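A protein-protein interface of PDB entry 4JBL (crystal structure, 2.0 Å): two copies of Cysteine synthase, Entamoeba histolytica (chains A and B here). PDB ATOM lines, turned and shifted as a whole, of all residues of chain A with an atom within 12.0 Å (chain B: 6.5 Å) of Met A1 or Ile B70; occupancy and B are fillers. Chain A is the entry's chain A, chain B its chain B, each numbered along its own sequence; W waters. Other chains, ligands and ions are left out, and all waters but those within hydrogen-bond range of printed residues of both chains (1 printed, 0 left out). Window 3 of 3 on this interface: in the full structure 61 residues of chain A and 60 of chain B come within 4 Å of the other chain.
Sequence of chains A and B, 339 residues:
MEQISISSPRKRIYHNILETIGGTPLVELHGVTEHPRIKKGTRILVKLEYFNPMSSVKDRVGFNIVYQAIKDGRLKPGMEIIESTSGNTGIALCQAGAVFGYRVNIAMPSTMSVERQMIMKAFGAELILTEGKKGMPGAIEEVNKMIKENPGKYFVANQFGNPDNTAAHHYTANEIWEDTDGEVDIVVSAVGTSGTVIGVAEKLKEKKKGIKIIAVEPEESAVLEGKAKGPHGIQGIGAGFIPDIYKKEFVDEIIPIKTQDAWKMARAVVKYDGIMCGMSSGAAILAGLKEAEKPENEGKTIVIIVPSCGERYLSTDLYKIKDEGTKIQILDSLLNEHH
The side-chain hydroxyl (OH) of Tyr B67 is in hydrogen-bond range of the backbone carbonyl oxygen (O) of Glu A2 (3.4 Å).
The side-chain hydroxyl of Tyr B67 sits at hydrogen-bond distance from the side-chain amide nitrogen of Gln A3 (3.3 Å).
The side-chain hydroxyl (OH) of Tyr B67 lies within hydrogen-bond range of the backbone NH (N) of Ile A4 (2.8 Å).
The side-chain amino group of Lys B71 is in hydrogen-bond range of the side-chain amide oxygen of Gln B68, at 3.4 Å.
Met A1 touches Tyr B67 (SD to CE1, 3.97 Å).
Met A1 touches Ile B70 (SD to CG2, 3.8 Å).
Met A1 touches Phe B100 (CE to CE1, 3.8 Å).
Lys B71 touches Gln A3.
Met A1 touches three residues of chain B.
Of the printed residues of chain B, Gln A3 touches Tyr B67 (3.3 Å) and Lys B71 (3.999 Å).
His A30 touches none of the printed residues of chain B.
Of chain A, only Met A1 (3.97 Å), Glu A2 (3.4 Å), Gln A3 (3.3 Å) and Ile A4 (2.8 Å) come within 4 Å of Tyr B67.
No residue of chain A comes within 4 Å of Ala B69.
Ile B70 touches just one residue of chain A: Met A1 (3.8 Å).
Printed residues of chain A within 4 Å of Lys B71: Gln A3 (3.999 Å).
No residue of chain A comes within 4 Å of Gly B73.
No residue of chain A comes within 4 Å of Leu B75.
Lys B76 touches none of the printed residues of chain A.
Of chain A, only Met A1 comes within 4 Å of Phe B100.
The nearest residue of chain B that does not touch Met A1 is Lys B71 (5.1 Å).
The nearest residue of chain A that does not touch Ile B70 is Glu A2 (8.2 Å).
Printed residues of chain B that touch a printed residue of chain A: Tyr B67, Ile B70, Lys B71 and Phe B100.
Of the 6 printed residues of chain A, 4 touch a printed residue of chain B.
Printed residues of chain A that touch a printed residue of chain B: Met A1, Glu A2, Gln A3 and Ile A4.
Hydrophobic or aromatic side chains of chain A within 4 Å of the printed part of chain B: Met A1 and Ile A4.
Among the printed residues, 7 pairs touch across the chains.
Among the printed residues, no Asp or Glu carboxylate lies within 4 Å of a Lys or Arg side-chain nitrogen of the other chain.
No position is printed for both chains.
Of the 7 pairs that touch across the chains among the printed residues, none has its exchanged pair printed and touching as well.
Water W1 bridges NE2 of Gln A3 (2.6 Å) and OH of Tyr B67 (2.7 Å).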
ATOM      1  N   MET A   1     -32.579 -13.342 -21.816  1.00  0.00           N
ATOM      2  CA  MET A   1     -32.035 -14.145 -22.955  1.00  0.00           C
ATOM      3  C   MET A   1     -33.192 -14.735 -23.777  1.00  0.00           C
ATOM      4  O   MET A   1     -34.138 -15.307 -23.201  1.00  0.00           O
ATOM      5  CB  MET A   1     -31.071 -15.249 -22.456  1.00  0.00           C
ATOM      6  CG  MET A   1     -31.715 -16.617 -22.214  1.00  0.00           C
ATOM      7  SD  MET A   1     -30.598 -18.040 -22.261  1.00  0.00           S
ATOM      8  CE  MET A   1     -29.335 -17.521 -23.431  1.00  0.00           C
ATOM      9  N   GLU A   2     -33.109 -14.576 -25.108  1.00  0.00           N
ATOM     10  CA  GLU A   2     -34.156 -15.043 -26.048  1.00  0.00           C
ATOM     11  C   GLU A   2     -34.567 -16.541 -25.964  1.00  0.00           C
ATOM     12  O   GLU A   2     -33.820 -17.413 -25.485  1.00  0.00           O
ATOM     13  CB  GLU A   2     -33.849 -14.598 -27.503  1.00  0.00           C
ATOM     14  CG  GLU A   2     -34.775 -13.490 -28.040  1.00  0.00           C
ATOM     15  CD  GLU A   2     -35.114 -12.370 -27.025  1.00  0.00           C
ATOM     16  OE1 GLU A   2     -34.344 -12.103 -26.068  1.00  0.00           O
ATOM     17  OE2 GLU A   2     -36.168 -11.723 -27.183  1.00  0.00           O
ATOM     18  N   GLN A   3     -35.791 -16.820 -26.373  1.00  0.00           N
ATOM     19  CA  GLN A   3     -36.189 -18.187 -26.481  1.00  0.00           C
ATOM     20  C   GLN A   3     -35.345 -18.707 -27.705  1.00  0.00           C
ATOM     21  O   GLN A   3     -35.144 -18.008 -28.692  1.00  0.00           O
ATOM     22  CB  GLN A   3     -37.736 -18.297 -26.597  1.00  0.00           C
ATOM     23  CG  GLN A   3     -38.558 -19.061 -25.499  1.00  0.00           C
ATOM     24  CD  GLN A   3     -38.283 -18.766 -23.968  1.00  0.00           C
ATOM     25  OE1 GLN A   3     -39.110 -18.156 -23.256  1.00  0.00           O
ATOM     26  NE2 GLN A   3     -37.149 -19.261 -23.455  1.00  0.00           N
ATOM     27  N   ILE A   4     -34.757 -19.889 -27.564  1.00  0.00           N
ATOM     28  CA  ILE A   4     -34.069 -20.570 -28.642  1.00  0.00           C
ATOM     29  C   ILE A   4     -35.000 -21.759 -28.949  1.00  0.00           C
ATOM     30  O   ILE A   4     -35.326 -22.511 -28.051  1.00  0.00           O
ATOM     31  CB  ILE A   4     -32.692 -21.078 -28.104  1.00  0.00           C
ATOM     32  CG1 ILE A   4     -31.797 -19.902 -27.718  1.00  0.00           C
ATOM     33  CG2 ILE A   4     -31.914 -21.914 -29.122  1.00  0.00           C
ATOM     34  CD1 ILE A   4     -31.690 -18.825 -28.814  1.00  0.00           C
ATOM     35  N   SER A   5     -35.448 -21.923 -30.182  1.00  0.00           N
ATOM     36  CA  SER A   5     -36.229 -23.113 -30.476  1.00  0.00           C
ATOM     37  C   SER A   5     -35.558 -23.915 -31.560  1.00  0.00           C
ATOM     38  O   SER A   5     -34.967 -23.361 -32.470  1.00  0.00           O
ATOM     39  CB  SER A   5     -37.621 -22.745 -30.932  1.00  0.00           C
ATOM     40  OG  SER A   5     -37.549 -21.435 -31.423  1.00  0.00           O
ATOM     41  N   HIS A  30     -22.896 -14.047 -35.077  1.00  0.00           N
ATOM     42  CA  HIS A  30     -23.031 -13.018 -33.996  1.00  0.00           C
ATOM     43  C   HIS A  30     -21.665 -12.903 -33.351  1.00  0.00           C
ATOM     44  O   HIS A  30     -21.043 -11.833 -33.361  1.00  0.00           O
ATOM     45  CB  HIS A  30     -24.103 -13.398 -32.970  1.00  0.00           C
ATOM     46  CG  HIS A  30     -25.483 -13.440 -33.547  1.00  0.00           C
ATOM     47  ND1 HIS A  30     -26.181 -12.320 -33.855  1.00  0.00           N
ATOM     48  CD2 HIS A  30     -26.287 -14.509 -33.892  1.00  0.00           C
ATOM     49  CE1 HIS A  30     -27.357 -12.662 -34.422  1.00  0.00           C
ATOM     50  NE2 HIS A  30     -27.447 -13.996 -34.396  1.00  0.00           N
ATOM     51  N   ILE B  65     -29.671 -29.912 -22.174  1.00  0.00           N
ATOM     52  CA  ILE B  65     -29.125 -29.986 -20.798  1.00  0.00           C
ATOM     53  C   ILE B  65     -28.592 -28.616 -20.393  1.00  0.00           C
ATOM     54  O   ILE B  65     -28.892 -28.107 -19.287  1.00  0.00           O
ATOM     55  CB  ILE B  65     -28.003 -31.062 -20.707  1.00  0.00           C
ATOM     56  CG1 ILE B  65     -28.641 -32.466 -20.654  1.00  0.00           C
ATOM     57  CG2 ILE B  65     -27.140 -30.894 -19.445  1.00  0.00           C
ATOM     58  CD1 ILE B  65     -27.585 -33.633 -20.549  1.00  0.00           C
ATOM     59  N   VAL B  66     -27.877 -27.970 -21.316  1.00  0.00           N
ATOM     60  CA  VAL B  66     -27.220 -26.739 -20.986  1.00  0.00           C
ATOM     61  C   VAL B  66     -28.252 -25.620 -20.974  1.00  0.00           C
ATOM     62  O   VAL B  66     -28.226 -24.765 -20.075  1.00  0.00           O
ATOM     63  CB  VAL B  66     -26.022 -26.438 -21.946  1.00  0.00           C
ATOM     64  CG1 VAL B  66     -25.491 -25.008 -21.745  1.00  0.00           C
ATOM     65  CG2 VAL B  66     -24.886 -27.463 -21.768  1.00  0.00           C
ATOM     66  N   TYR B  67     -29.138 -25.589 -21.967  1.00  0.00           N
ATOM     67  CA  TYR B  67     -30.077 -24.474 -22.087  1.00  0.00           C
ATOM     68  C   TYR B  67     -31.042 -24.540 -20.894  1.00  0.00           C
ATOM     69  O   TYR B  67     -31.417 -23.499 -20.352  1.00  0.00           O
ATOM     70  CB  TYR B  67     -30.845 -24.635 -23.355  1.00  0.00           C
ATOM     71  CG  TYR B  67     -31.783 -23.555 -23.717  1.00  0.00           C
ATOM     72  CD1 TYR B  67     -31.546 -22.222 -23.391  1.00  0.00           C
ATOM     73  CD2 TYR B  67     -32.919 -23.865 -24.426  1.00  0.00           C
ATOM     74  CE1 TYR B  67     -32.458 -21.210 -23.765  1.00  0.00           C
ATOM     75  CE2 TYR B  67     -33.818 -22.895 -24.812  1.00  0.00           C
ATOM     76  CZ  TYR B  67     -33.587 -21.576 -24.482  1.00  0.00           C
ATOM     77  OH  TYR B  67     -34.564 -20.708 -24.909  1.00  0.00           O
ATOM     78  N   GLN B  68     -31.509 -25.735 -20.518  1.00  0.00           N
ATOM     79  CA  GLN B  68     -32.402 -25.764 -19.373  1.00  0.00           C
ATOM     80  C   GLN B  68     -31.656 -25.369 -18.111  1.00  0.00           C
ATOM     81  O   GLN B  68     -32.205 -24.678 -17.266  1.00  0.00           O
ATOM     82  CB  GLN B  68     -33.097 -27.132 -19.139  1.00  0.00           C
ATOM     83  CG  GLN B  68     -33.910 -27.554 -20.359  1.00  0.00           C
ATOM     84  CD  GLN B  68     -35.289 -26.854 -20.496  1.00  0.00           C
ATOM     85  OE1 GLN B  68     -35.716 -26.056 -19.617  1.00  0.00           O
ATOM     86  NE2 GLN B  68     -36.001 -27.183 -21.592  1.00  0.00           N
ATOM     87  N   ALA B  69     -30.423 -25.817 -17.959  1.00  0.00           N
ATOM     88  CA  ALA B  69     -29.690 -25.487 -16.758  1.00  0.00           C
ATOM     89  C   ALA B  69     -29.475 -23.980 -16.605  1.00  0.00           C
ATOM     90  O   ALA B  69     -29.466 -23.443 -15.480  1.00  0.00           O
ATOM     91  CB  ALA B  69     -28.383 -26.215 -16.729  1.00  0.00           C
ATOM     92  N   ILE B  70     -29.279 -23.289 -17.722  1.00  0.00           N
ATOM     93  CA  ILE B  70     -29.187 -21.838 -17.733  1.00  0.00           C
ATOM     94  C   ILE B  70     -30.567 -21.197 -17.422  1.00  0.00           C
ATOM     95  O   ILE B  70     -30.631 -20.263 -16.614  1.00  0.00           O
ATOM     96  CB  ILE B  70     -28.647 -21.325 -19.112  1.00  0.00           C
ATOM     97  CG1 ILE B  70     -27.182 -21.662 -19.302  1.00  0.00           C
ATOM     98  CG2 ILE B  70     -28.922 -19.818 -19.332  1.00  0.00           C
ATOM     99  CD1 ILE B  70     -26.734 -21.433 -20.774  1.00  0.00           C
ATOM    100  N   LYS B  71     -31.636 -21.657 -18.025  1.00  0.00           N
ATOM    101  CA  LYS B  71     -32.940 -21.143 -17.722  1.00  0.00           C
ATOM    102  C   LYS B  71     -33.286 -21.411 -16.244  1.00  0.00           C
ATOM    103  O   LYS B  71     -33.860 -20.585 -15.610  1.00  0.00           O
ATOM    104  CB  LYS B  71     -33.990 -21.699 -18.651  1.00  0.00           C
ATOM    105  CG  LYS B  71     -33.984 -21.132 -20.053  1.00  0.00           C
ATOM    106  CD  LYS B  71     -35.108 -21.612 -20.945  1.00  0.00           C
ATOM    107  CE  LYS B  71     -35.040 -23.083 -21.245  1.00  0.00           C
ATOM    108  NZ  LYS B  71     -36.166 -23.663 -21.997  1.00  0.00           N
ATOM    109  N   ASP B  72     -32.865 -22.552 -15.735  1.00  0.00           N
ATOM    110  CA  ASP B  72     -33.074 -23.014 -14.371  1.00  0.00           C
ATOM    111  C   ASP B  72     -32.381 -22.239 -13.298  1.00  0.00           C
ATOM    112  O   ASP B  72     -32.935 -22.038 -12.302  1.00  0.00           O
ATOM    113  CB  ASP B  72     -32.734 -24.521 -14.203  1.00  0.00           C
ATOM    114  CG  ASP B  72     -33.837 -25.338 -14.631  1.00  0.00           C
ATOM    115  OD1 ASP B  72     -34.791 -24.663 -14.969  1.00  0.00           O
ATOM    116  OD2 ASP B  72     -33.824 -26.542 -14.679  1.00  0.00           O
ATOM    117  N   GLY B  73     -31.155 -21.864 -13.497  1.00  0.00           N
ATOM    118  CA  GLY B  73     -30.359 -21.308 -12.455  1.00  0.00           C
ATOM    119  C   GLY B  73     -29.303 -22.275 -12.080  1.00  0.00           C
ATOM    120  O   GLY B  73     -28.418 -21.941 -11.361  1.00  0.00           O
ATOM    121  N   ARG B  74     -29.397 -23.491 -12.599  1.00  0.00           N
ATOM    122  CA  ARG B  74     -28.369 -24.487 -12.317  1.00  0.00           C
ATOM    123  C   ARG B  74     -27.009 -24.240 -13.005  1.00  0.00           C
ATOM    124  O   ARG B  74     -26.001 -24.742 -12.605  1.00  0.00           O
ATOM    125  CB  ARG B  74     -28.883 -25.887 -12.628  1.00  0.00           C
ATOM    126  CG  ARG B  74     -30.067 -26.375 -11.797  1.00  0.00           C
ATOM    127  CD  ARG B  74     -30.584 -27.741 -12.188  1.00  0.00           C
ATOM    128  NE  ARG B  74     -31.455 -27.680 -13.331  1.00  0.00           N
ATOM    129  CZ  ARG B  74     -31.289 -28.381 -14.423  1.00  0.00           C
ATOM    130  NH1 ARG B  74     -30.292 -29.215 -14.492  1.00  0.00           N
ATOM    131  NH2 ARG B  74     -32.096 -28.239 -15.439  1.00  0.00           N
ATOM    132  N   LEU B  75     -27.021 -23.444 -14.052  1.00  0.00           N
ATOM    133  CA  LEU B  75     -25.811 -23.009 -14.709  1.00  0.00           C
ATOM    134  C   LEU B  75     -25.847 -21.500 -14.786  1.00  0.00           C
ATOM    135  O   LEU B  75     -26.753 -20.938 -15.348  1.00  0.00           O
ATOM    136  CB  LEU B  75     -25.704 -23.594 -16.105  1.00  0.00           C
ATOM    137  CG  LEU B  75     -24.438 -23.254 -16.875  1.00  0.00           C
ATOM    138  CD1 LEU B  75     -23.149 -23.542 -16.157  1.00  0.00           C
ATOM    139  CD2 LEU B  75     -24.437 -23.882 -18.245  1.00  0.00           C
ATOM    140  N   LYS B  76     -24.884 -20.827 -14.237  1.00  0.00           N
ATOM    141  CA  LYS B  76     -25.041 -19.369 -14.134  1.00  0.00           C
ATOM    142  C   LYS B  76     -23.735 -18.685 -14.457  1.00  0.00           C
ATOM    143  O   LYS B  76     -22.639 -19.286 -14.311  1.00  0.00           O
ATOM    144  CB  LYS B  76     -25.519 -18.973 -12.735  1.00  0.00           C
ATOM    145  CG  LYS B  76     -24.541 -19.319 -11.623  1.00  0.00           C
ATOM    146  CD  LYS B  76     -25.043 -18.834 -10.274  1.00  0.00           C
ATOM    147  CE  LYS B  76     -24.170 -19.346  -9.141  1.00  0.00           C
ATOM    148  NZ  LYS B  76     -22.765 -18.868  -9.264  1.00  0.00           N
ATOM    149  N   ALA B  96     -22.928 -26.371 -27.519  1.00  0.00           N
ATOM    150  CA  ALA B  96     -23.776 -25.511 -26.657  1.00  0.00           C
ATOM    151  C   ALA B  96     -22.947 -24.515 -25.829  1.00  0.00           C
ATOM    152  O   ALA B  96     -23.336 -23.322 -25.687  1.00  0.00           O
ATOM    153  CB  ALA B  96     -24.676 -26.382 -25.763  1.00  0.00           C
ATOM    154  N   PHE B 100     -23.391 -20.430 -25.905  1.00  0.00           N
ATOM    155  CA  PHE B 100     -23.852 -19.773 -24.690  1.00  0.00           C
ATOM    156  C   PHE B 100     -22.747 -19.033 -23.902  1.00  0.00           C
ATOM    157  O   PHE B 100     -23.036 -18.202 -23.107  1.00  0.00           O
ATOM    158  CB  PHE B 100     -24.562 -20.749 -23.759  1.00  0.00           C
ATOM    159  CG  PHE B 100     -25.897 -21.234 -24.244  1.00  0.00           C
ATOM    160  CD1 PHE B 100     -26.961 -20.397 -24.402  1.00  0.00           C
ATOM    161  CD2 PHE B 100     -26.084 -22.554 -24.484  1.00  0.00           C
ATOM    162  CE1 PHE B 100     -28.151 -20.860 -24.851  1.00  0.00           C
ATOM    163  CE2 PHE B 100     -27.261 -23.031 -24.922  1.00  0.00           C
ATOM    164  CZ  PHE B 100     -28.304 -22.189 -25.111  1.00  0.00           C
ATOM    165  N   TYR B 102     -19.888 -20.641 -22.237  1.00  0.00           N
ATOM    166  CA  TYR B 102     -19.395 -21.339 -21.073  1.00  0.00           C
ATOM    167  C   TYR B 102     -18.278 -22.314 -21.439  1.00  0.00           C
ATOM    168  O   TYR B 102     -18.308 -22.953 -22.468  1.00  0.00           O
ATOM    169  CB  TYR B 102     -20.560 -22.062 -20.384  1.00  0.00           C
ATOM    170  CG  TYR B 102     -21.558 -21.189 -19.680  1.00  0.00           C
ATOM    171  CD1 TYR B 102     -21.516 -21.045 -18.305  1.00  0.00           C
ATOM    172  CD2 TYR B 102     -22.553 -20.570 -20.342  1.00  0.00           C
ATOM    173  CE1 TYR B 102     -22.419 -20.283 -17.645  1.00  0.00           C
ATOM    174  CE2 TYR B 102     -23.461 -19.794 -19.681  1.00  0.00           C
ATOM    175  CZ  TYR B 102     -23.361 -19.653 -18.322  1.00  0.00           C
ATOM    176  OH  TYR B 102     -24.220 -18.891 -17.655  1.00  0.00           O
HETATM  177  O   HOH W   1     -37.094 -21.540 -24.675  1.00  0.00           O
